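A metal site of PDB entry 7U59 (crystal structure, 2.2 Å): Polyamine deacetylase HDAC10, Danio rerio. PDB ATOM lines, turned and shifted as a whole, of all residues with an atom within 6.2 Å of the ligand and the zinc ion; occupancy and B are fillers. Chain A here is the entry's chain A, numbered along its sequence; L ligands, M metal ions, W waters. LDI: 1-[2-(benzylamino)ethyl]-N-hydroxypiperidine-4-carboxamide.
A ring nitrogen (NE2) of His 136 lies close to an oxygen (O01) of the ligand (2.6 Å). The side-chain hydroxyl (OH) of Tyr 307 lies close to an oxygen (O04) of the ligand (2.6 Å). A nitrogen (N02) of the ligand is in hydrogen-bond range of a ring nitrogen (NE2) of His 137 (2.7 Å). The side-chain carboxylate (OE2) of Glu 24 lies within salt-bridge range of a nitrogen (N11) of the ligand (2.9 Å).
The side-chain carboxylate of Asp 174 is in hydrogen-bond range of the backbone NH of Gly 305. OD1 of Asp 267 lies within hydrogen-bond range of N of Val 175 (2.9 Å). A ring nitrogen (NE2) of His 137 sits at hydrogen-bond distance from a ring nitrogen (NE2) of His 136 (3.2 Å). The side-chain sulfur (SG) of Cys 147 lies within hydrogen-bond range of the backbone NH (N) of His 137 (3.5 Å). The side-chain amide oxygen (OD1) of Asn 93 sits at hydrogen-bond distance from the indole nitrogen (NE1) of Trp 205. The backbone carbonyl oxygen of Ala 94 sits at hydrogen-bond distance from the backbone NH of Phe 146 (2.8 Å). The backbone NH (N) of Gly 145 sits at hydrogen-bond distance from the backbone carbonyl oxygen (O) of Asn 93 (3.0 Å). The backbone carbonyl oxygen (O) of Gly 145 sits at hydrogen-bond distance from the side-chain sulfur (SG) of Cys 147 (3.5 Å).
Gly 145 touches the ligand. Phe 146 touches the ligand (CE2 to C06, 3.7 Å). CD1 of Trp 205 touches C12 of the ligand, 3.4 Å away. Glu 274 touches the ligand (OE1 to C07, 3.9 Å). Hydrophobic or aromatic side chains within 4 Å of the ligand: His 136, His 137, Phe 146, His 176, Trp 205 and Tyr 307. Of the 22 residues printed, 11 come within 4 Å of the ligand. Along chain A the residues within 4 Å of the ligand span positions 24 to 307.
OD2 of Asp 174 is bound to the zinc ion, 1.9 Å away. The zinc ion is bound by OD2 of Asp 267, at 2.0 Å. O01 of the ligand binds the zinc ion (2.2 Å). O04 of the ligand binds the zinc ion, 2.3 Å away. ND1 of His 176 is bound to the zinc ion (2.3 Å). The zinc ion has five donor atoms within binding distance. Slightly farther from the zinc ion lies OD1 of Asp 174 (2.6 Å).
Water W1 bridges OE1 of Glu 274 (2.5 Å) and NE2 of His 176 (2.6 Å).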
ATOM      1  N   GLU A  24      26.149 -32.465  -5.211  1.00  0.00           N
ATOM      2  CA  GLU A  24      26.374 -31.981  -3.846  1.00  0.00           C
ATOM      3  C   GLU A  24      25.110 -31.345  -3.254  1.00  0.00           C
ATOM      4  O   GLU A  24      24.795 -31.561  -2.077  1.00  0.00           O
ATOM      5  CB  GLU A  24      27.538 -30.991  -3.840  1.00  0.00           C
ATOM      6  CG  GLU A  24      27.794 -30.400  -2.482  1.00  0.00           C
ATOM      7  CD  GLU A  24      28.948 -29.418  -2.480  1.00  0.00           C
ATOM      8  OE1 GLU A  24      29.188 -28.741  -3.513  1.00  0.00           O
ATOM      9  OE2 GLU A  24      29.611 -29.316  -1.425  1.00  0.00           O
ATOM     10  N   ILE A  27      20.409 -33.030  -2.636  1.00  0.00           N
ATOM     11  CA  ILE A  27      19.693 -33.596  -1.484  1.00  0.00           C
ATOM     12  C   ILE A  27      18.779 -32.586  -0.809  1.00  0.00           C
ATOM     13  O   ILE A  27      17.955 -32.973   0.032  1.00  0.00           O
ATOM     14  CB  ILE A  27      20.659 -34.107  -0.406  1.00  0.00           C
ATOM     15  CG1 ILE A  27      21.680 -33.009  -0.082  1.00  0.00           C
ATOM     16  CG2 ILE A  27      21.342 -35.406  -0.839  1.00  0.00           C
ATOM     17  CD1 ILE A  27      22.452 -33.248   1.177  1.00  0.00           C
ATOM     18  N   ASN A  93      30.211 -21.678  -1.100  1.00  0.00           N
ATOM     19  CA  ASN A  93      30.490 -23.095  -0.890  1.00  0.00           C
ATOM     20  C   ASN A  93      29.198 -23.847  -0.598  1.00  0.00           C
ATOM     21  O   ASN A  93      28.518 -23.553   0.389  1.00  0.00           O
ATOM     22  CB  ASN A  93      31.475 -23.258   0.276  1.00  0.00           C
ATOM     23  CG  ASN A  93      32.185 -24.584   0.212  1.00  0.00           C
ATOM     24  OD1 ASN A  93      31.560 -25.645   0.305  1.00  0.00           O
ATOM     25  ND2 ASN A  93      33.501 -24.541   0.034  1.00  0.00           N
ATOM     26  N   ALA A  94      28.881 -24.833  -1.449  1.00  0.00           N
ATOM     27  CA  ALA A  94      27.789 -25.781  -1.218  1.00  0.00           C
ATOM     28  C   ALA A  94      26.433 -25.081  -1.057  1.00  0.00           C
ATOM     29  O   ALA A  94      25.726 -25.210  -0.050  1.00  0.00           O
ATOM     30  CB  ALA A  94      28.093 -26.669   0.001  1.00  0.00           C
ATOM     31  N   PRO A 134      17.595 -23.597   5.257  1.00  0.00           N
ATOM     32  CA  PRO A 134      18.148 -23.612   6.615  1.00  0.00           C
ATOM     33  C   PRO A 134      19.059 -22.416   6.847  1.00  0.00           C
ATOM     34  O   PRO A 134      19.274 -21.623   5.926  1.00  0.00           O
ATOM     35  CB  PRO A 134      18.928 -24.939   6.669  1.00  0.00           C
ATOM     36  CG  PRO A 134      19.351 -25.172   5.240  1.00  0.00           C
ATOM     37  CD  PRO A 134      18.220 -24.609   4.379  1.00  0.00           C
ATOM     38  N   HIS A 136      22.087 -22.267   9.638  1.00  0.00           N
ATOM     39  CA  HIS A 136      23.138 -22.190  10.650  1.00  0.00           C
ATOM     40  C   HIS A 136      24.555 -22.070  10.054  1.00  0.00           C
ATOM     41  O   HIS A 136      25.456 -21.634  10.759  1.00  0.00           O
ATOM     42  CB  HIS A 136      23.045 -23.364  11.652  1.00  0.00           C
ATOM     43  CG  HIS A 136      23.400 -24.716  11.098  1.00  0.00           C
ATOM     44  ND1 HIS A 136      23.908 -25.727  11.901  1.00  0.00           N
ATOM     45  CD2 HIS A 136      23.298 -25.239   9.862  1.00  0.00           C
ATOM     46  CE1 HIS A 136      24.115 -26.806  11.164  1.00  0.00           C
ATOM     47  NE2 HIS A 136      23.741 -26.543   9.931  1.00  0.00           N
ATOM     48  N   HIS A 137      24.728 -22.360   8.775  1.00  0.00           N
ATOM     49  CA  HIS A 137      25.998 -22.102   8.102  1.00  0.00           C
ATOM     50  C   HIS A 137      26.156 -20.678   7.559  1.00  0.00           C
ATOM     51  O   HIS A 137      27.282 -20.273   7.267  1.00  0.00           O
ATOM     52  CB  HIS A 137      26.171 -23.060   6.936  1.00  0.00           C
ATOM     53  CG  HIS A 137      26.247 -24.491   7.353  1.00  0.00           C
ATOM     54  ND1 HIS A 137      27.120 -24.920   8.333  1.00  0.00           N
ATOM     55  CD2 HIS A 137      25.557 -25.582   6.948  1.00  0.00           C
ATOM     56  CE1 HIS A 137      26.956 -26.212   8.522  1.00  0.00           C
ATOM     57  NE2 HIS A 137      26.025 -26.641   7.687  1.00  0.00           N
ATOM     58  N   GLY A 145      26.494 -23.782   2.570  1.00  0.00           N
ATOM     59  CA  GLY A 145      25.884 -25.031   2.986  1.00  0.00           C
ATOM     60  C   GLY A 145      24.364 -25.007   2.994  1.00  0.00           C
ATOM     61  O   GLY A 145      23.765 -25.296   4.029  1.00  0.00           O
ATOM     62  N   PHE A 146      23.744 -24.619   1.866  1.00  0.00           N
ATOM     63  CA  PHE A 146      22.298 -24.523   1.680  1.00  0.00           C
ATOM     64  C   PHE A 146      21.674 -23.328   2.396  1.00  0.00           C
ATOM     65  O   PHE A 146      20.474 -23.084   2.221  1.00  0.00           O
ATOM     66  CB  PHE A 146      21.550 -25.784   2.157  1.00  0.00           C
ATOM     67  CG  PHE A 146      22.017 -27.045   1.518  1.00  0.00           C
ATOM     68  CD1 PHE A 146      22.686 -27.017   0.306  1.00  0.00           C
ATOM     69  CD2 PHE A 146      21.793 -28.275   2.123  1.00  0.00           C
ATOM     70  CE1 PHE A 146      23.122 -28.178  -0.289  1.00  0.00           C
ATOM     71  CE2 PHE A 146      22.184 -29.435   1.518  1.00  0.00           C
ATOM     72  CZ  PHE A 146      22.869 -29.380   0.305  1.00  0.00           C
ATOM     73  N   CYS A 147      22.449 -22.592   3.194  1.00  0.00           N
ATOM     74  CA  CYS A 147      21.929 -21.536   4.051  1.00  0.00           C
ATOM     75  C   CYS A 147      22.132 -20.171   3.393  1.00  0.00           C
ATOM     76  O   CYS A 147      23.226 -19.889   2.900  1.00  0.00           O
ATOM     77  CB  CYS A 147      22.633 -21.549   5.407  1.00  0.00           C
ATOM     78  SG  CYS A 147      22.413 -23.080   6.305  1.00  0.00           S
ATOM     79  N   ASP A 174      21.895 -30.489  14.714  1.00  0.00           N
ATOM     80  CA  ASP A 174      22.237 -30.851  13.347  1.00  0.00           C
ATOM     81  C   ASP A 174      23.586 -31.555  13.356  1.00  0.00           C
ATOM     82  O   ASP A 174      24.420 -31.299  14.237  1.00  0.00           O
ATOM     83  CB  ASP A 174      22.278 -29.595  12.455  1.00  0.00           C
ATOM     84  CG  ASP A 174      22.399 -29.895  10.964  1.00  0.00           C
ATOM     85  OD1 ASP A 174      21.374 -29.808  10.253  1.00  0.00           O
ATOM     86  OD2 ASP A 174      23.511 -30.159  10.458  1.00  0.00           O
ATOM     87  N   VAL A 175      23.798 -32.459  12.392  1.00  0.00           N
ATOM     88  CA  VAL A 175      25.043 -33.226  12.362  1.00  0.00           C
ATOM     89  C   VAL A 175      26.218 -32.409  11.846  1.00  0.00           C
ATOM     90  O   VAL A 175      27.366 -32.859  11.924  1.00  0.00           O
ATOM     91  CB  VAL A 175      24.858 -34.496  11.515  1.00  0.00           C
ATOM     92  CG1 VAL A 175      25.083 -34.199  10.013  1.00  0.00           C
ATOM     93  CG2 VAL A 175      25.785 -35.600  11.997  1.00  0.00           C
ATOM     94  N   HIS A 176      25.963 -31.246  11.272  1.00  0.00           N
ATOM     95  CA  HIS A 176      26.994 -30.351  10.774  1.00  0.00           C
ATOM     96  C   HIS A 176      27.248 -29.234  11.783  1.00  0.00           C
ATOM     97  O   HIS A 176      26.365 -28.865  12.554  1.00  0.00           O
ATOM     98  CB  HIS A 176      26.597 -29.742   9.422  1.00  0.00           C
ATOM     99  CG  HIS A 176      26.521 -30.733   8.305  1.00  0.00           C
ATOM    100  ND1 HIS A 176      25.353 -31.394   7.947  1.00  0.00           N
ATOM    101  CD2 HIS A 176      27.480 -31.176   7.442  1.00  0.00           C
ATOM    102  CE1 HIS A 176      25.595 -32.186   6.916  1.00  0.00           C
ATOM    103  NE2 HIS A 176      26.873 -32.072   6.592  1.00  0.00           N
ATOM    104  N   HIS A 177      28.456 -28.695  11.757  1.00  0.00           N
ATOM    105  CA  HIS A 177      28.811 -27.601  12.651  1.00  0.00           C
ATOM    106  C   HIS A 177      28.191 -26.287  12.166  1.00  0.00           C
ATOM    107  O   HIS A 177      28.403 -25.897  11.015  1.00  0.00           O
ATOM    108  CB  HIS A 177      30.325 -27.434  12.728  1.00  0.00           C
ATOM    109  CG  HIS A 177      30.759 -26.311  13.628  1.00  0.00           C
ATOM    110  ND1 HIS A 177      31.742 -25.410  13.288  1.00  0.00           N
ATOM    111  CD2 HIS A 177      30.340 -25.969  14.869  1.00  0.00           C
ATOM    112  CE1 HIS A 177      31.901 -24.541  14.272  1.00  0.00           C
ATOM    113  NE2 HIS A 177      31.078 -24.867  15.252  1.00  0.00           N
ATOM    114  N   TRP A 205      33.126 -31.924   6.035  1.00  0.00           N
ATOM    115  CA  TRP A 205      32.674 -30.570   5.741  1.00  0.00           C
ATOM    116  C   TRP A 205      32.047 -29.947   6.987  1.00  0.00           C
ATOM    117  O   TRP A 205      31.285 -30.620   7.701  1.00  0.00           O
ATOM    118  CB  TRP A 205      31.668 -30.617   4.578  1.00  0.00           C
ATOM    119  CG  TRP A 205      31.413 -29.280   3.961  1.00  0.00           C
ATOM    120  CD1 TRP A 205      32.052 -28.745   2.876  1.00  0.00           C
ATOM    121  CD2 TRP A 205      30.467 -28.304   4.399  1.00  0.00           C
ATOM    122  NE1 TRP A 205      31.559 -27.487   2.618  1.00  0.00           N
ATOM    123  CE2 TRP A 205      30.595 -27.187   3.547  1.00  0.00           C
ATOM    124  CE3 TRP A 205      29.531 -28.253   5.451  1.00  0.00           C
ATOM    125  CZ2 TRP A 205      29.818 -26.034   3.696  1.00  0.00           C
ATOM    126  CZ3 TRP A 205      28.765 -27.091   5.605  1.00  0.00           C
ATOM    127  CH2 TRP A 205      28.913 -26.000   4.728  1.00  0.00           C
ATOM    128  N   GLY A 265      18.600 -29.887  13.171  1.00  0.00           N
ATOM    129  CA  GLY A 265      18.816 -30.635  11.949  1.00  0.00           C
ATOM    130  C   GLY A 265      18.697 -32.106  12.294  1.00  0.00           C
ATOM    131  O   GLY A 265      19.224 -32.560  13.309  1.00  0.00           O
ATOM    132  N   ASP A 267      19.611 -34.492  10.201  1.00  0.00           N
ATOM    133  CA  ASP A 267      20.630 -35.290   9.551  1.00  0.00           C
ATOM    134  C   ASP A 267      21.554 -35.960  10.555  1.00  0.00           C
ATOM    135  O   ASP A 267      22.436 -36.712  10.135  1.00  0.00           O
ATOM    136  CB  ASP A 267      21.439 -34.467   8.531  1.00  0.00           C
ATOM    137  CG  ASP A 267      21.958 -33.145   9.073  1.00  0.00           C
ATOM    138  OD1 ASP A 267      21.912 -32.893  10.297  1.00  0.00           O
ATOM    139  OD2 ASP A 267      22.447 -32.346   8.239  1.00  0.00           O
ATOM    140  N   GLU A 274      24.032 -37.768   4.780  1.00  0.00           N
ATOM    141  CA  GLU A 274      25.125 -36.867   5.080  1.00  0.00           C
ATOM    142  C   GLU A 274      25.750 -37.148   6.438  1.00  0.00           C
ATOM    143  O   GLU A 274      26.981 -37.107   6.576  1.00  0.00           O
ATOM    144  CB  GLU A 274      24.651 -35.415   5.029  1.00  0.00           C
ATOM    145  CG  GLU A 274      24.297 -34.939   3.646  1.00  0.00           C
ATOM    146  CD  GLU A 274      25.453 -35.115   2.652  1.00  0.00           C
ATOM    147  OE1 GLU A 274      26.592 -34.706   2.973  1.00  0.00           O
ATOM    148  OE2 GLU A 274      25.203 -35.660   1.546  1.00  0.00           O
ATOM    149  N   GLU A 304      16.765 -27.155  10.598  1.00  0.00           N
ATOM    150  CA  GLU A 304      17.955 -26.943   9.784  1.00  0.00           C
ATOM    151  C   GLU A 304      17.970 -28.018   8.707  1.00  0.00           C
ATOM    152  O   GLU A 304      17.175 -27.947   7.756  1.00  0.00           O
ATOM    153  CB  GLU A 304      19.197 -26.912  10.670  1.00  0.00           C
ATOM    154  CG  GLU A 304      19.178 -25.786  11.727  1.00  0.00           C
ATOM    155  CD  GLU A 304      19.668 -24.442  11.154  1.00  0.00           C
ATOM    156  OE1 GLU A 304      20.000 -24.391   9.957  1.00  0.00           O
ATOM    157  OE2 GLU A 304      19.781 -23.455  11.916  1.00  0.00           O
ATOM    158  N   GLY A 305      18.847 -29.027   8.805  1.00  0.00           N
ATOM    159  CA  GLY A 305      18.951 -30.064   7.782  1.00  0.00           C
ATOM    160  C   GLY A 305      18.167 -31.334   8.105  1.00  0.00           C
ATOM    161  O   GLY A 305      17.329 -31.380   9.010  1.00  0.00           O
ATOM    162  N   GLY A 306      18.472 -32.390   7.337  1.00  0.00           N
ATOM    163  CA  GLY A 306      17.803 -33.687   7.471  1.00  0.00           C
ATOM    164  C   GLY A 306      17.300 -34.148   6.115  1.00  0.00           C
ATOM    165  O   GLY A 306      16.420 -33.504   5.537  1.00  0.00           O
ATOM    166  N   TYR A 307      17.842 -35.244   5.573  1.00  0.00           N
ATOM    167  CA  TYR A 307      17.719 -35.517   4.146  1.00  0.00           C
ATOM    168  C   TYR A 307      17.191 -36.899   3.802  1.00  0.00           C
ATOM    169  O   TYR A 307      16.946 -37.169   2.628  1.00  0.00           O
ATOM    170  CB  TYR A 307      19.083 -35.330   3.451  1.00  0.00           C
ATOM    171  CG  TYR A 307      19.626 -33.970   3.776  1.00  0.00           C
ATOM    172  CD1 TYR A 307      19.099 -32.851   3.138  1.00  0.00           C
ATOM    173  CD2 TYR A 307      20.596 -33.799   4.751  1.00  0.00           C
ATOM    174  CE1 TYR A 307      19.542 -31.581   3.445  1.00  0.00           C
ATOM    175  CE2 TYR A 307      21.058 -32.521   5.069  1.00  0.00           C
ATOM    176  CZ  TYR A 307      20.532 -31.419   4.414  1.00  0.00           C
ATOM    177  OH  TYR A 307      20.967 -30.152   4.700  1.00  0.00           O
HETATM  178  C10 LDI L   1      28.714 -30.445   1.736  1.00  0.00           C
HETATM  179  C13 LDI L   1      31.546 -31.977  -0.345  1.00  0.00           C
HETATM  180  C15 LDI L   1      32.359 -32.230  -2.608  1.00  0.00           C
HETATM  181  C17 LDI L   1      32.684 -33.996  -1.022  1.00  0.00           C
HETATM  182  C20 LDI L   1      25.684 -28.720   4.486  1.00  0.00           C
HETATM  183  C03 LDI L   1      23.799 -29.409   5.946  1.00  0.00           C
HETATM  184  C05 LDI L   1      24.429 -29.439   4.518  1.00  0.00           C
HETATM  185  C06 LDI L   1      24.533 -30.802   4.044  1.00  0.00           C
HETATM  186  C07 LDI L   1      25.356 -30.971   2.747  1.00  0.00           C
HETATM  187  C09 LDI L   1      27.179 -30.371   1.631  1.00  0.00           C
HETATM  188  C12 LDI L   1      30.817 -31.147   0.736  1.00  0.00           C
HETATM  189  C14 LDI L   1      31.718 -31.481  -1.634  1.00  0.00           C
HETATM  190  C16 LDI L   1      32.850 -33.496  -2.304  1.00  0.00           C
HETATM  191  C18 LDI L   1      32.036 -33.247  -0.054  1.00  0.00           C
HETATM  192  C19 LDI L   1      26.671 -29.006   3.325  1.00  0.00           C
HETATM  193  N02 LDI L   1      24.137 -28.392   6.897  1.00  0.00           N
HETATM  194  N08 LDI L   1      26.654 -30.327   2.737  1.00  0.00           N
HETATM  195  N11 LDI L   1      29.352 -31.283   0.711  1.00  0.00           N
HETATM  196  O01 LDI L   1      23.545 -28.396   8.175  1.00  0.00           O
HETATM  197  O04 LDI L   1      23.024 -30.230   6.317  1.00  0.00           O
HETATM  198 ZN    ZN M   1      23.297 -30.538   8.583  1.00  0.00          ZN
HETATM  199  O   HOH W   1      27.637 -32.840   4.226  1.00  0.00           O
HETATM  200  O   HOH W   2      28.552 -33.550  -0.344  1.00  0.00           O
HETATM  201  O   HOH W   3      30.218 -33.532   2.953  1.00  0.00           O
